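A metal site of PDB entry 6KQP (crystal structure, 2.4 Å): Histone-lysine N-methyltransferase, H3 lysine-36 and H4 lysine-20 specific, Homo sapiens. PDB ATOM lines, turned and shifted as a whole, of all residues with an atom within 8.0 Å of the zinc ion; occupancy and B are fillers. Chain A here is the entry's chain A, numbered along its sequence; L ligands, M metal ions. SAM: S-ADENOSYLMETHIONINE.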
ATOM      1  N   ARG A  89      25.349  10.425  18.471  1.00  0.00           N
ATOM      2  CA  ARG A  89      24.078   9.670  18.345  1.00  0.00           C
ATOM      3  C   ARG A  89      24.279   8.456  17.435  1.00  0.00           C
ATOM      4  O   ARG A  89      23.283   7.965  16.861  1.00  0.00           O
ATOM      5  CB  ARG A  89      22.984  10.606  17.812  1.00  0.00           C
ATOM      6  CG  ARG A  89      22.459  11.581  18.869  1.00  0.00           C
ATOM      7  CD  ARG A  89      21.655  12.725  18.269  1.00  0.00           C
ATOM      8  NE  ARG A  89      22.398  13.377  17.210  1.00  0.00           N
ATOM      9  CZ  ARG A  89      22.043  13.424  15.935  1.00  0.00           C
ATOM     10  NH1 ARG A  89      20.908  12.892  15.509  1.00  0.00           N
ATOM     11  NH2 ARG A  89      22.857  14.037  15.070  1.00  0.00           N
ATOM     12  N   HIS A 158      16.232  10.044  17.311  1.00  0.00           N
ATOM     13  CA  HIS A 158      15.268  10.905  18.017  1.00  0.00           C
ATOM     14  C   HIS A 158      15.790  12.337  18.039  1.00  0.00           C
ATOM     15  O   HIS A 158      17.012  12.549  18.256  1.00  0.00           O
ATOM     16  CB  HIS A 158      15.026  10.430  19.430  1.00  0.00           C
ATOM     17  CG  HIS A 158      14.345  11.448  20.254  1.00  0.00           C
ATOM     18  ND1 HIS A 158      12.985  11.451  20.415  1.00  0.00           N
ATOM     19  CD2 HIS A 158      14.840  12.476  20.969  1.00  0.00           C
ATOM     20  CE1 HIS A 158      12.661  12.445  21.231  1.00  0.00           C
ATOM     21  NE2 HIS A 158      13.784  13.108  21.582  1.00  0.00           N
ATOM     22  N   CYS A 159      14.868  13.275  17.883  1.00  0.00           N
ATOM     23  CA  CYS A 159      15.081  14.721  18.130  1.00  0.00           C
ATOM     24  C   CYS A 159      13.803  15.276  18.771  1.00  0.00           C
ATOM     25  O   CYS A 159      12.699  14.910  18.295  1.00  0.00           O
ATOM     26  CB  CYS A 159      15.484  15.431  16.844  1.00  0.00           C
ATOM     27  SG  CYS A 159      15.590  17.236  16.961  1.00  0.00           S
ATOM     28  N   CYS A 160      13.961  16.093  19.808  1.00  0.00           N
ATOM     29  CA  CYS A 160      12.851  16.738  20.561  1.00  0.00           C
ATOM     30  C   CYS A 160      12.218  17.883  19.751  1.00  0.00           C
ATOM     31  O   CYS A 160      11.106  18.240  20.114  1.00  0.00           O
ATOM     32  CB  CYS A 160      13.332  17.266  21.900  1.00  0.00           C
ATOM     33  SG  CYS A 160      13.914  15.990  23.051  1.00  0.00           S
ATOM     34  N   GLN A 161      12.854  18.409  18.709  1.00  0.00           N
ATOM     35  CA  GLN A 161      12.215  19.311  17.687  1.00  0.00           C
ATOM     36  C   GLN A 161      12.503  18.736  16.307  1.00  0.00           C
ATOM     37  O   GLN A 161      13.388  19.180  15.583  1.00  0.00           O
ATOM     38  CB  GLN A 161      12.695  20.752  17.774  1.00  0.00           C
ATOM     39  N   ASN A 194      10.506  12.513  16.679  1.00  0.00           N
ATOM     40  CA  ASN A 194      10.303  12.411  18.129  1.00  0.00           C
ATOM     41  C   ASN A 194       9.727  11.025  18.428  1.00  0.00           C
ATOM     42  O   ASN A 194       8.666  10.715  17.914  1.00  0.00           O
ATOM     43  CB  ASN A 194       9.337  13.487  18.614  1.00  0.00           C
ATOM     44  CG  ASN A 194       9.315  13.647  20.113  1.00  0.00           C
ATOM     45  OD1 ASN A 194       9.476  12.688  20.872  1.00  0.00           O
ATOM     46  ND2 ASN A 194       9.100  14.872  20.553  1.00  0.00           N
ATOM     47  N   VAL A 206      20.500   9.492  27.595  1.00  0.00           N
ATOM     48  CA  VAL A 206      20.501  10.984  27.590  1.00  0.00           C
ATOM     49  C   VAL A 206      20.389  11.418  26.134  1.00  0.00           C
ATOM     50  O   VAL A 206      21.205  10.984  25.295  1.00  0.00           O
ATOM     51  CB  VAL A 206      21.765  11.565  28.257  1.00  0.00           C
ATOM     52  CG1 VAL A 206      21.894  13.063  28.044  1.00  0.00           C
ATOM     53  CG2 VAL A 206      21.821  11.241  29.747  1.00  0.00           C
ATOM     54  N   CYS A 207      19.417  12.279  25.851  1.00  0.00           N
ATOM     55  CA  CYS A 207      19.201  12.800  24.477  1.00  0.00           C
ATOM     56  C   CYS A 207      20.365  13.734  24.124  1.00  0.00           C
ATOM     57  O   CYS A 207      20.696  14.605  24.928  1.00  0.00           O
ATOM     58  CB  CYS A 207      17.847  13.483  24.353  1.00  0.00           C
ATOM     59  SG  CYS A 207      17.486  13.923  22.643  1.00  0.00           S
ATOM     60  N   LYS A 208      20.928  13.555  22.936  1.00  0.00           N
ATOM     61  CA  LYS A 208      21.927  14.480  22.340  1.00  0.00           C
ATOM     62  C   LYS A 208      21.360  15.097  21.050  1.00  0.00           C
ATOM     63  O   LYS A 208      22.157  15.292  20.144  1.00  0.00           O
ATOM     64  CB  LYS A 208      23.220  13.722  22.021  1.00  0.00           C
ATOM     65  CG  LYS A 208      23.860  12.998  23.197  1.00  0.00           C
ATOM     66  CD  LYS A 208      24.262  13.907  24.329  1.00  0.00           C
ATOM     67  CE  LYS A 208      24.994  13.176  25.435  1.00  0.00           C
ATOM     68  NZ  LYS A 208      25.211  14.035  26.624  1.00  0.00           N
ATOM     69  N   CYS A 209      20.052  15.353  20.960  1.00  0.00           N
ATOM     70  CA  CYS A 209      19.415  15.851  19.704  1.00  0.00           C
ATOM     71  C   CYS A 209      19.964  17.246  19.327  1.00  0.00           C
ATOM     72  O   CYS A 209      20.049  17.533  18.113  1.00  0.00           O
ATOM     73  CB  CYS A 209      17.891  15.849  19.772  1.00  0.00           C
ATOM     74  SG  CYS A 209      17.130  17.029  20.925  1.00  0.00           S
ATOM     75  N   GLY A 210      20.318  18.086  20.295  1.00  0.00           N
ATOM     76  CA  GLY A 210      20.858  19.430  20.049  1.00  0.00           C
ATOM     77  C   GLY A 210      19.760  20.450  19.828  1.00  0.00           C
ATOM     78  O   GLY A 210      20.093  21.563  19.390  1.00  0.00           O
ATOM     79  N   ALA A 211      18.499  20.095  20.109  1.00  0.00           N
ATOM     80  CA  ALA A 211      17.337  20.996  19.955  1.00  0.00           C
ATOM     81  C   ALA A 211      17.227  21.912  21.157  1.00  0.00           C
ATOM     82  O   ALA A 211      17.435  21.475  22.280  1.00  0.00           O
ATOM     83  CB  ALA A 211      16.069  20.209  19.766  1.00  0.00           C
ATOM     84  N   PRO A 212      16.876  23.205  20.948  1.00  0.00           N
ATOM     85  CA  PRO A 212      16.679  24.163  22.051  1.00  0.00           C
ATOM     86  C   PRO A 212      15.693  23.706  23.147  1.00  0.00           C
ATOM     87  O   PRO A 212      15.948  24.004  24.274  1.00  0.00           O
ATOM     88  CB  PRO A 212      16.112  25.405  21.349  1.00  0.00           C
ATOM     89  CG  PRO A 212      16.655  25.315  19.930  1.00  0.00           C
ATOM     90  CD  PRO A 212      16.666  23.827  19.628  1.00  0.00           C
ATOM     91  N   ASN A 213      14.642  22.984  22.783  1.00  0.00           N
ATOM     92  CA  ASN A 213      13.592  22.517  23.736  1.00  0.00           C
ATOM     93  C   ASN A 213      13.890  21.090  24.222  1.00  0.00           C
ATOM     94  O   ASN A 213      12.956  20.455  24.747  1.00  0.00           O
ATOM     95  CB  ASN A 213      12.191  22.577  23.093  1.00  0.00           C
ATOM     96  CG  ASN A 213      12.079  21.842  21.769  1.00  0.00           C
ATOM     97  OD1 ASN A 213      12.837  22.118  20.832  1.00  0.00           O
ATOM     98  ND2 ASN A 213      11.117  20.938  21.658  1.00  0.00           N
ATOM     99  N   CYS A 214      15.125  20.601  24.101  1.00  0.00           N
ATOM    100  CA  CYS A 214      15.479  19.187  24.393  1.00  0.00           C
ATOM    101  C   CYS A 214      15.160  18.829  25.850  1.00  0.00           C
ATOM    102  O   CYS A 214      15.655  19.498  26.759  1.00  0.00           O
ATOM    103  CB  CYS A 214      16.945  18.892  24.084  1.00  0.00           C
ATOM    104  SG  CYS A 214      17.421  17.199  24.505  1.00  0.00           S
ATOM    105  N   SER A 215      14.406  17.741  26.061  1.00  0.00           N
ATOM    106  CA  SER A 215      13.972  17.265  27.403  1.00  0.00           C
ATOM    107  C   SER A 215      15.101  16.462  28.074  1.00  0.00           C
ATOM    108  O   SER A 215      14.963  16.125  29.269  1.00  0.00           O
ATOM    109  CB  SER A 215      12.731  16.437  27.251  1.00  0.00           C
ATOM    110  OG  SER A 215      13.070  15.120  26.862  1.00  0.00           O
ATOM    111  N   GLY A 216      16.162  16.120  27.328  1.00  0.00           N
ATOM    112  CA  GLY A 216      17.231  15.219  27.784  1.00  0.00           C
ATOM    113  C   GLY A 216      16.846  13.735  27.751  1.00  0.00           C
ATOM    114  O   GLY A 216      17.693  12.907  28.106  1.00  0.00           O
ATOM    115  N   PHE A 217      15.636  13.382  27.310  1.00  0.00           N
ATOM    116  CA  PHE A 217      15.188  11.984  27.137  1.00  0.00           C
ATOM    117  C   PHE A 217      14.764  11.722  25.693  1.00  0.00           C
ATOM    118  O   PHE A 217      14.451  12.653  24.948  1.00  0.00           O
ATOM    119  CB  PHE A 217      14.027  11.660  28.082  1.00  0.00           C
ATOM    120  CG  PHE A 217      14.402  11.697  29.537  1.00  0.00           C
ATOM    121  CD1 PHE A 217      15.076  10.625  30.117  1.00  0.00           C
ATOM    122  CD2 PHE A 217      14.087  12.793  30.331  1.00  0.00           C
ATOM    123  CE1 PHE A 217      15.425  10.646  31.471  1.00  0.00           C
ATOM    124  CE2 PHE A 217      14.416  12.801  31.682  1.00  0.00           C
ATOM    125  CZ  PHE A 217      15.081  11.730  32.251  1.00  0.00           C
ATOM    126  N   LEU A 218      14.784  10.449  25.300  1.00  0.00           N
ATOM    127  CA  LEU A 218      14.255  10.003  23.975  1.00  0.00           C
ATOM    128  C   LEU A 218      12.749   9.758  24.143  1.00  0.00           C
ATOM    129  O   LEU A 218      12.349   8.588  24.359  1.00  0.00           O
ATOM    130  CB  LEU A 218      14.988   8.740  23.521  1.00  0.00           C
ATOM    131  CG  LEU A 218      16.295   8.945  22.744  1.00  0.00           C
ATOM    132  CD1 LEU A 218      17.216   9.918  23.438  1.00  0.00           C
ATOM    133  CD2 LEU A 218      16.988   7.609  22.520  1.00  0.00           C
ATOM    134  N   GLY A 219      11.954  10.844  24.132  1.00  0.00           N
ATOM    135  CA  GLY A 219      10.487  10.763  24.260  1.00  0.00           C
ATOM    136  C   GLY A 219       9.981  10.596  25.696  1.00  0.00           C
ATOM    137  O   GLY A 219       9.066  11.338  26.056  1.00  0.00           O
HETATM  138  N   SAM L   1      21.912   5.802  16.070  1.00  0.00           N
HETATM  139  CA  SAM L   1      21.274   4.481  15.826  1.00  0.00           C
HETATM  140  C   SAM L   1      22.335   3.517  15.276  1.00  0.00           C
HETATM  141  O   SAM L   1      23.526   3.760  15.569  1.00  0.00           O
HETATM  142  OXT SAM L   1      21.952   2.544  14.594  1.00  0.00           O
HETATM  143  CB  SAM L   1      20.091   4.637  14.855  1.00  0.00           C
HETATM  144  CG  SAM L   1      18.807   5.035  15.573  1.00  0.00           C
HETATM  145  SD  SAM L   1      18.141   3.646  16.533  1.00  0.00           S
HETATM  146  CE  SAM L   1      16.447   3.577  15.925  1.00  0.00           C
HETATM  147  C5' SAM L   1      17.829   4.414  18.117  1.00  0.00           C
HETATM  148  C4' SAM L   1      19.015   4.382  19.047  1.00  0.00           C
HETATM  149  O4' SAM L   1      19.969   5.408  18.651  1.00  0.00           O
HETATM  150  C3' SAM L   1      18.625   4.664  20.492  1.00  0.00           C
HETATM  151  O3' SAM L   1      18.404   3.437  21.165  1.00  0.00           O
HETATM  152  C2' SAM L   1      19.833   5.453  21.012  1.00  0.00           C
HETATM  153  O2' SAM L   1      20.800   4.584  21.549  1.00  0.00           O
HETATM  154  C1' SAM L   1      20.339   6.185  19.763  1.00  0.00           C
HETATM  155  N9  SAM L   1      19.755   7.509  19.625  1.00  0.00           N
HETATM  156  C8  SAM L   1      18.742   7.870  18.761  1.00  0.00           C
HETATM  157  N7  SAM L   1      18.380   9.126  18.873  1.00  0.00           N
HETATM  158  C5  SAM L   1      19.187   9.618  19.885  1.00  0.00           C
HETATM  159  C6  SAM L   1      19.272  10.894  20.497  1.00  0.00           C
HETATM  160  N6  SAM L   1      18.517  11.927  20.157  1.00  0.00           N
HETATM  161  N1  SAM L   1      20.164  11.045  21.504  1.00  0.00           N
HETATM  162  C2  SAM L   1      20.935   9.997  21.838  1.00  0.00           C
HETATM  163  N3  SAM L   1      20.948   8.759  21.344  1.00  0.00           N
HETATM  164  C4  SAM L   1      20.028   8.628  20.363  1.00  0.00           C
HETATM  165 ZN    ZN M   1      16.393  16.051  22.698  1.00  0.00          ZN
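The zinc ion is bound by the side-chain sulfur of Cys 209, the side-chain sulfur of Cys 214, the side-chain sulfur of Cys 207 and the side-chain sulfur of Cys 160.
Within 4 Å of the zinc ion: Cys 160, Cys 207, Cys 209 and Cys 214.
The backbone NH (N) of Ala 211 sits close to the side-chain sulfur (SG) of Cys 209 (3.5 Å).
SG of Cys 214 lies close to N of Gly 216, 3.3 Å away.
N of Cys 207 is in hydrogen-bond range of O of Gly 216 (2.9 Å).
The backbone NH (N) of Cys 160 sits at hydrogen-bond distance from a ring nitrogen (NE2) of His 158.
N of Ser 215 lies close to SG of Cys 160 (3.5 Å).
The backbone carbonyl oxygen (O) of Cys 160 sits at hydrogen-bond distance from the side-chain amide nitrogen (ND2) of Asn 213 (3.1 Å).
N6 of the ligand sits close to SG of Cys 207, 3.4 Å away.
The backbone NH (N) of His 158 lies within hydrogen-bond range of a nitrogen (N7) of the ligand, at 2.8 Å.
The backbone carbonyl oxygen of His 158 is in hydrogen-bond range of a nitrogen (N6) of the ligand, 2.5 Å away.
N of Lys 208 lies within hydrogen-bond range of N1 of the ligand, 3.0 Å away.
A nitrogen (N) of the ligand lies within hydrogen-bond range of the backbone carbonyl oxygen of Arg 89, 2.7 Å away.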
